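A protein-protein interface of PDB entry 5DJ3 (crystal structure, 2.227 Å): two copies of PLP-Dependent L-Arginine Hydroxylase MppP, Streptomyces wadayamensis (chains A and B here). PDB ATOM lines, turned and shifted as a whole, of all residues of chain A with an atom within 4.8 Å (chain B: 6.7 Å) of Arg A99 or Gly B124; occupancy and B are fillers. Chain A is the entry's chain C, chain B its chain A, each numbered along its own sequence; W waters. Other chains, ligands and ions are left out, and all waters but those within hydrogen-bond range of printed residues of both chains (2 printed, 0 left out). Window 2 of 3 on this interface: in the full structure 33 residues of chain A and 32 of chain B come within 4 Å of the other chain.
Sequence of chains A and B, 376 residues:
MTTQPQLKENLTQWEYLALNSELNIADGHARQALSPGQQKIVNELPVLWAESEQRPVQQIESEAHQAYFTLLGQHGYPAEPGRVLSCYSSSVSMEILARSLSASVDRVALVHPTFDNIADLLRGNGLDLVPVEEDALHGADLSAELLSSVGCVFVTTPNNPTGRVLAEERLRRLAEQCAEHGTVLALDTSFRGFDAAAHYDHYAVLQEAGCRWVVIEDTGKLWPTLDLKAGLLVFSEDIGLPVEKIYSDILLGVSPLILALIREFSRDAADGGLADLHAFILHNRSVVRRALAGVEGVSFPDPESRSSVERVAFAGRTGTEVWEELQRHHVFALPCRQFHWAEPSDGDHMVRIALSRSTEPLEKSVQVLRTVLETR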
ATOM      1  N   GLU A  95      14.403 -32.942   5.037  1.00  0.00           N
ATOM      2  CA  GLU A  95      14.171 -31.868   4.081  1.00  0.00           C
ATOM      3  C   GLU A  95      14.852 -30.602   4.558  1.00  0.00           C
ATOM      4  O   GLU A  95      15.525 -29.915   3.779  1.00  0.00           O
ATOM      5  CB  GLU A  95      12.658 -31.640   3.915  1.00  0.00           C
ATOM      6  CG  GLU A  95      12.205 -30.478   3.020  1.00  0.00           C
ATOM      7  CD  GLU A  95      12.371 -30.731   1.516  1.00  0.00           C
ATOM      8  OE1 GLU A  95      12.729 -31.846   1.106  1.00  0.00           O
ATOM      9  OE2 GLU A  95      12.137 -29.792   0.734  1.00  0.00           O
ATOM     10  N   ILE A  96      14.708 -30.300   5.851  1.00  0.00           N
ATOM     11  CA  ILE A  96      15.366 -29.138   6.434  1.00  0.00           C
ATOM     12  C   ILE A  96      16.882 -29.248   6.269  1.00  0.00           C
ATOM     13  O   ILE A  96      17.537 -28.294   5.851  1.00  0.00           O
ATOM     14  CB  ILE A  96      14.954 -28.979   7.908  1.00  0.00           C
ATOM     15  CG1 ILE A  96      13.500 -28.481   8.014  1.00  0.00           C
ATOM     16  CG2 ILE A  96      15.933 -28.021   8.667  1.00  0.00           C
ATOM     17  CD1 ILE A  96      12.877 -28.819   9.435  1.00  0.00           C
ATOM     18  N   LEU A  97      17.447 -30.429   6.550  1.00  0.00           N
ATOM     19  CA  LEU A  97      18.889 -30.654   6.396  1.00  0.00           C
ATOM     20  C   LEU A  97      19.354 -30.568   4.936  1.00  0.00           C
ATOM     21  O   LEU A  97      20.415 -29.997   4.664  1.00  0.00           O
ATOM     22  CB  LEU A  97      19.271 -32.025   6.967  1.00  0.00           C
ATOM     23  CG  LEU A  97      20.730 -32.474   6.803  1.00  0.00           C
ATOM     24  CD1 LEU A  97      21.737 -31.609   7.545  1.00  0.00           C
ATOM     25  CD2 LEU A  97      20.893 -33.904   7.283  1.00  0.00           C
ATOM     26  N   ALA A  98      18.640 -31.223   3.996  1.00  0.00           N
ATOM     27  CA  ALA A  98      19.060 -31.199   2.592  1.00  0.00           C
ATOM     28  C   ALA A  98      19.066 -29.770   2.056  1.00  0.00           C
ATOM     29  O   ALA A  98      20.030 -29.318   1.426  1.00  0.00           O
ATOM     30  CB  ALA A  98      18.143 -32.070   1.719  1.00  0.00           C
ATOM     31  N   ARG A  99      18.002 -29.033   2.326  1.00  0.00           N
ATOM     32  CA  ARG A  99      17.968 -27.664   1.865  1.00  0.00           C
ATOM     33  C   ARG A  99      19.020 -26.824   2.576  1.00  0.00           C
ATOM     34  O   ARG A  99      19.641 -25.971   1.949  1.00  0.00           O
ATOM     35  CB  ARG A  99      16.566 -27.110   2.044  1.00  0.00           C
ATOM     36  CG  ARG A  99      16.378 -25.898   1.225  1.00  0.00           C
ATOM     37  CD  ARG A  99      15.087 -25.932   0.476  1.00  0.00           C
ATOM     38  NE  ARG A  99      13.943 -25.709   1.338  1.00  0.00           N
ATOM     39  CZ  ARG A  99      13.741 -24.613   2.073  1.00  0.00           C
ATOM     40  NH1 ARG A  99      14.632 -23.615   2.111  1.00  0.00           N
ATOM     41  NH2 ARG A  99      12.649 -24.541   2.814  1.00  0.00           N
ATOM     42  N   SER A 100      19.297 -27.115   3.849  1.00  0.00           N
ATOM     43  CA  SER A 100      20.326 -26.387   4.566  1.00  0.00           C
ATOM     44  C   SER A 100      21.710 -26.680   4.010  1.00  0.00           C
ATOM     45  O   SER A 100      22.603 -25.829   4.093  1.00  0.00           O
ATOM     46  CB  SER A 100      20.275 -26.742   6.065  1.00  0.00           C
ATOM     47  OG  SER A 100      19.172 -26.112   6.728  1.00  0.00           O
ATOM     48  N   LEU A 101      21.905 -27.884   3.464  1.00  0.00           N
ATOM     49  CA  LEU A 101      23.174 -28.245   2.851  1.00  0.00           C
ATOM     50  C   LEU A 101      23.358 -27.576   1.499  1.00  0.00           C
ATOM     51  O   LEU A 101      24.484 -27.266   1.128  1.00  0.00           O
ATOM     52  CB  LEU A 101      23.266 -29.761   2.680  1.00  0.00           C
ATOM     53  CG  LEU A 101      23.461 -30.591   3.927  1.00  0.00           C
ATOM     54  CD1 LEU A 101      23.182 -32.002   3.551  1.00  0.00           C
ATOM     55  CD2 LEU A 101      24.862 -30.451   4.473  1.00  0.00           C
ATOM     56  N   SER A 102      22.276 -27.363   0.741  1.00  0.00           N
ATOM     57  CA  SER A 102      22.428 -27.115  -0.688  1.00  0.00           C
ATOM     58  C   SER A 102      23.111 -25.793  -1.028  1.00  0.00           C
ATOM     59  O   SER A 102      23.689 -25.695  -2.115  1.00  0.00           O
ATOM     60  CB  SER A 102      21.062 -27.203  -1.378  1.00  0.00           C
ATOM     61  OG  SER A 102      20.181 -26.191  -0.944  1.00  0.00           O
ATOM     62  N   ALA A 103      23.091 -24.788  -0.143  1.00  0.00           N
ATOM     63  CA  ALA A 103      23.806 -23.529  -0.428  1.00  0.00           C
ATOM     64  C   ALA A 103      25.313 -23.743  -0.551  1.00  0.00           C
ATOM     65  O   ALA A 103      25.959 -23.207  -1.465  1.00  0.00           O
ATOM     66  CB  ALA A 103      23.540 -22.499   0.665  1.00  0.00           C
ATOM     67  N   ASN A 125      16.942 -31.611  -3.680  1.00  0.00           N
ATOM     68  CA  ASN A 125      17.374 -30.288  -3.269  1.00  0.00           C
ATOM     69  C   ASN A 125      18.695 -29.868  -3.911  1.00  0.00           C
ATOM     70  O   ASN A 125      19.324 -28.913  -3.439  1.00  0.00           O
ATOM     71  CB  ASN A 125      17.473 -30.212  -1.750  1.00  0.00           C
ATOM     72  CG  ASN A 125      16.088 -30.072  -1.096  1.00  0.00           C
ATOM     73  OD1 ASN A 125      15.447 -29.032  -1.218  1.00  0.00           O
ATOM     74  ND2 ASN A 125      15.609 -31.142  -0.457  1.00  0.00           N
ATOM     75  N   ILE A 246      15.791 -22.545   8.608  1.00  0.00           N
ATOM     76  CA  ILE A 246      14.877 -23.226   7.697  1.00  0.00           C
ATOM     77  C   ILE A 246      13.851 -24.026   8.492  1.00  0.00           C
ATOM     78  O   ILE A 246      12.696 -24.160   8.077  1.00  0.00           O
ATOM     79  CB  ILE A 246      15.665 -24.115   6.693  1.00  0.00           C
ATOM     80  CG1 ILE A 246      16.453 -23.232   5.678  1.00  0.00           C
ATOM     81  CG2 ILE A 246      14.726 -25.091   5.955  1.00  0.00           C
ATOM     82  CD1 ILE A 246      17.323 -23.996   4.701  1.00  0.00           C
ATOM     83  N   ILE A 250       9.586 -23.741   8.528  1.00  0.00           N
ATOM     84  CA  ILE A 250       8.641 -24.814   8.278  1.00  0.00           C
ATOM     85  C   ILE A 250       7.715 -25.033   9.470  1.00  0.00           C
ATOM     86  O   ILE A 250       6.521 -25.269   9.280  1.00  0.00           O
ATOM     87  CB  ILE A 250       9.375 -26.100   7.853  1.00  0.00           C
ATOM     88  CG1 ILE A 250       9.998 -25.868   6.466  1.00  0.00           C
ATOM     89  CG2 ILE A 250       8.392 -27.242   7.777  1.00  0.00           C
ATOM     90  CD1 ILE A 250      10.795 -26.968   5.911  1.00  0.00           C
ATOM     91  N   GLU B  95       6.059 -26.076   1.508  1.00  0.00           N
ATOM     92  CA  GLU B  95       7.379 -26.536   1.099  1.00  0.00           C
ATOM     93  C   GLU B  95       7.284 -27.423  -0.132  1.00  0.00           C
ATOM     94  O   GLU B  95       8.065 -27.276  -1.070  1.00  0.00           O
ATOM     95  CB  GLU B  95       8.024 -27.306   2.248  1.00  0.00           C
ATOM     96  CG  GLU B  95       9.304 -27.988   1.891  1.00  0.00           C
ATOM     97  CD  GLU B  95      10.445 -27.009   1.722  1.00  0.00           C
ATOM     98  OE1 GLU B  95      10.210 -25.794   1.904  1.00  0.00           O
ATOM     99  OE2 GLU B  95      11.567 -27.443   1.385  1.00  0.00           O
ATOM    100  N   ALA B  98       6.380 -25.133  -3.076  1.00  0.00           N
ATOM    101  CA  ALA B  98       7.526 -24.310  -3.464  1.00  0.00           C
ATOM    102  C   ALA B  98       8.512 -25.136  -4.273  1.00  0.00           C
ATOM    103  O   ALA B  98       8.898 -24.766  -5.387  1.00  0.00           O
ATOM    104  CB  ALA B  98       8.245 -23.700  -2.239  1.00  0.00           C
ATOM    105  N   ARG B  99       8.956 -26.254  -3.705  1.00  0.00           N
ATOM    106  CA  ARG B  99       9.942 -27.070  -4.410  1.00  0.00           C
ATOM    107  C   ARG B  99       9.379 -27.593  -5.737  1.00  0.00           C
ATOM    108  O   ARG B  99      10.116 -27.701  -6.717  1.00  0.00           O
ATOM    109  CB  ARG B  99      10.417 -28.211  -3.513  1.00  0.00           C
ATOM    110  CG  ARG B  99      11.584 -28.963  -4.116  1.00  0.00           C
ATOM    111  CD  ARG B  99      12.646 -29.212  -3.113  1.00  0.00           C
ATOM    112  NE  ARG B  99      12.332 -30.258  -2.141  1.00  0.00           N
ATOM    113  CZ  ARG B  99      12.353 -31.567  -2.403  1.00  0.00           C
ATOM    114  NH1 ARG B  99      12.593 -31.991  -3.632  1.00  0.00           N
ATOM    115  NH2 ARG B  99      12.102 -32.462  -1.441  1.00  0.00           N
ATOM    116  N   ALA B 119       6.689 -16.556   1.827  1.00  0.00           N
ATOM    117  CA  ALA B 119       7.806 -15.956   1.106  1.00  0.00           C
ATOM    118  C   ALA B 119       9.115 -16.676   1.398  1.00  0.00           C
ATOM    119  O   ALA B 119       9.908 -16.929   0.478  1.00  0.00           O
ATOM    120  CB  ALA B 119       7.935 -14.467   1.473  1.00  0.00           C
ATOM    121  N   ASP B 120       9.394 -16.979   2.677  1.00  0.00           N
ATOM    122  CA  ASP B 120      10.682 -17.605   2.958  1.00  0.00           C
ATOM    123  C   ASP B 120      10.775 -19.005   2.333  1.00  0.00           C
ATOM    124  O   ASP B 120      11.845 -19.398   1.867  1.00  0.00           O
ATOM    125  CB  ASP B 120      10.958 -17.644   4.464  1.00  0.00           C
ATOM    126  CG  ASP B 120      11.082 -16.264   5.073  1.00  0.00           C
ATOM    127  OD1 ASP B 120      11.148 -15.289   4.302  1.00  0.00           O
ATOM    128  OD2 ASP B 120      11.149 -16.169   6.326  1.00  0.00           O
ATOM    129  N   LEU B 121       9.671 -19.753   2.267  1.00  0.00           N
ATOM    130  CA  LEU B 121       9.716 -21.061   1.617  1.00  0.00           C
ATOM    131  C   LEU B 121       9.916 -20.940   0.104  1.00  0.00           C
ATOM    132  O   LEU B 121      10.721 -21.681  -0.489  1.00  0.00           O
ATOM    133  CB  LEU B 121       8.455 -21.841   1.960  1.00  0.00           C
ATOM    134  CG  LEU B 121       8.401 -22.231   3.452  1.00  0.00           C
ATOM    135  CD1 LEU B 121       7.028 -22.759   3.885  1.00  0.00           C
ATOM    136  CD2 LEU B 121       9.459 -23.206   3.767  1.00  0.00           C
ATOM    137  N   LEU B 122       9.219 -19.997  -0.535  1.00  0.00           N
ATOM    138  CA  LEU B 122       9.365 -19.834  -1.972  1.00  0.00           C
ATOM    139  C   LEU B 122      10.749 -19.335  -2.320  1.00  0.00           C
ATOM    140  O   LEU B 122      11.403 -19.843  -3.247  1.00  0.00           O
ATOM    141  CB  LEU B 122       8.330 -18.858  -2.504  1.00  0.00           C
ATOM    142  CG  LEU B 122       6.914 -19.371  -2.507  1.00  0.00           C
ATOM    143  CD1 LEU B 122       5.984 -18.227  -2.748  1.00  0.00           C
ATOM    144  CD2 LEU B 122       6.787 -20.432  -3.597  1.00  0.00           C
ATOM    145  N   ARG B 123      11.199 -18.315  -1.599  1.00  0.00           N
ATOM    146  CA  ARG B 123      12.502 -17.757  -1.892  1.00  0.00           C
ATOM    147  C   ARG B 123      13.579 -18.802  -1.625  1.00  0.00           C
ATOM    148  O   ARG B 123      14.501 -18.985  -2.436  1.00  0.00           O
ATOM    149  CB  ARG B 123      12.674 -16.467  -1.075  1.00  0.00           C
ATOM    150  CG  ARG B 123      13.968 -15.727  -1.231  1.00  0.00           C
ATOM    151  CD  ARG B 123      13.718 -14.240  -0.991  1.00  0.00           C
ATOM    152  NE  ARG B 123      12.994 -13.995   0.254  1.00  0.00           N
ATOM    153  CZ  ARG B 123      12.141 -12.992   0.449  1.00  0.00           C
ATOM    154  NH1 ARG B 123      11.872 -12.125  -0.520  1.00  0.00           N
ATOM    155  NH2 ARG B 123      11.547 -12.863   1.621  1.00  0.00           N
ATOM    156  N   GLY B 124      13.414 -19.569  -0.544  1.00  0.00           N
ATOM    157  CA  GLY B 124      14.374 -20.603  -0.162  1.00  0.00           C
ATOM    158  C   GLY B 124      14.412 -21.791  -1.106  1.00  0.00           C
ATOM    159  O   GLY B 124      15.430 -22.484  -1.178  1.00  0.00           O
ATOM    160  N   ASN B 125      13.343 -22.025  -1.859  1.00  0.00           N
ATOM    161  CA  ASN B 125      13.367 -23.001  -2.933  1.00  0.00           C
ATOM    162  C   ASN B 125      13.710 -22.393  -4.289  1.00  0.00           C
ATOM    163  O   ASN B 125      13.581 -23.075  -5.311  1.00  0.00           O
ATOM    164  CB  ASN B 125      12.027 -23.704  -2.992  1.00  0.00           C
ATOM    165  CG  ASN B 125      11.904 -24.742  -1.954  1.00  0.00           C
ATOM    166  OD1 ASN B 125      12.401 -25.823  -2.145  1.00  0.00           O
ATOM    167  ND2 ASN B 125      11.252 -24.425  -0.831  1.00  0.00           N
ATOM    168  N   GLY B 126      14.142 -21.135  -4.327  1.00  0.00           N
ATOM    169  CA  GLY B 126      14.747 -20.591  -5.522  1.00  0.00           C
ATOM    170  C   GLY B 126      13.835 -19.799  -6.431  1.00  0.00           C
ATOM    171  O   GLY B 126      14.250 -19.468  -7.540  1.00  0.00           O
ATOM    172  N   LEU B 127      12.611 -19.486  -5.989  1.00  0.00           N
ATOM    173  CA  LEU B 127      11.679 -18.656  -6.736  1.00  0.00           C
ATOM    174  C   LEU B 127      11.929 -17.173  -6.469  1.00  0.00           C
ATOM    175  O   LEU B 127      12.131 -16.744  -5.322  1.00  0.00           O
ATOM    176  CB  LEU B 127      10.244 -18.999  -6.351  1.00  0.00           C
ATOM    177  CG  LEU B 127       9.634 -20.359  -6.731  1.00  0.00           C
ATOM    178  CD1 LEU B 127       9.842 -20.655  -8.210  1.00  0.00           C
ATOM    179  CD2 LEU B 127      10.191 -21.517  -5.900  1.00  0.00           C
HETATM  180  O   HOH W   1      14.823 -26.494  -3.547  1.00  0.00           O
HETATM  181  O   HOH W   2      12.949 -21.336   3.414  1.00  0.00           O
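Water W2 bridges the backbone carbonyl oxygen of Asp B120 (2.7 Å) and the guanidinium group of Arg A99 (3.1 Å).
OE2 of Glu B95 sits close to OE2 of Glu A95 (2.5 Å). The side-chain carboxylate of Glu B95 lies within salt-bridge range of the guanidinium group of Arg A99. The side-chain carboxylate (OE1) of Glu A95 lies within salt-bridge range of the guanidinium group (NH2) of Arg B99. The guanidinium group (NE) of Arg B99 lies close to the side-chain amide oxygen (OD1) of Asn A125 (3.5 Å).
Glu B95 touches its own counterpart, Glu A95. Glu A95 touches Arg B99, and with the chains exchanged Arg A99 touches Glu B95. Arg A99 touches Asn B125, and with the chains exchanged Asn A125 touches Arg B99.
The side-chain carboxylate (OE1) of Glu B95 is in hydrogen-bond range of the side-chain amide nitrogen (ND2) of Asn B125 (3.2 Å). The side-chain amide nitrogen (ND2) of Asn B125 sits at hydrogen-bond distance from the backbone carbonyl oxygen (O) of Leu B121 (2.8 Å). The side-chain carboxylate (OE1) of Glu A95 is in hydrogen-bond range of the side-chain amide nitrogen (ND2) of Asn A125 (3.4 Å). The backbone carbonyl oxygen of Arg A99 is in hydrogen-bond range of the side-chain hydroxyl of Ser A102 (3.0 Å).
Among the printed residues, pairs that only touch across the chains: Arg A99 with Gly B124, Arg A99 with Leu B121, Arg A99 with Asn B125 and Ile A250 with Leu B121.
Of the 12 printed residues of chain A, 4 touch a printed residue of chain B. Hydrophobic or aromatic side chains of chain A that line the printed part of chain B: Ile A250. Along chain A the printed residues that touch a printed residue of chain B span positions 95 to 250. Hydrophobic or aromatic side chains of chain B that line the printed part of chain A: Leu B121. Among the printed residues, 8 pairs touch across the chains. Among the printed residues, Asp or Glu carboxylates within 4 Å of a Lys or Arg side-chain nitrogen of the other chain: Glu A95 with Arg B99 and Arg A99 with Glu B95.
Arg A99 touches just these residues of chain B: Glu B95 (2.9 Å), Leu B121 (3.6 Å), Gly B124 (3.6 Å) and Asn B125 (3.7 Å). Of the printed residues of chain A, Gly B124 touches Arg A99. Printed residues of chain A within 4 Å of Glu B95: Glu A95 (2.5 Å) and Arg A99 (2.9 Å). Printed residues of chain B within 4 Å of Glu A95: Glu B95 (2.5 Å) and Arg B99 (2.7 Å). Printed residues of chain B within 4 Å of Ile A250: Leu B121. Leu A101 touches none of the printed residues of chain B. Arg B123 touches none of the printed residues of chain A. The nearest residue of chain B that does not touch Arg A99 is Asp B120 (5.1 Å). The nearest printed residue of chain A that does not touch Gly B124 is Ser A102 (6.0 Å).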
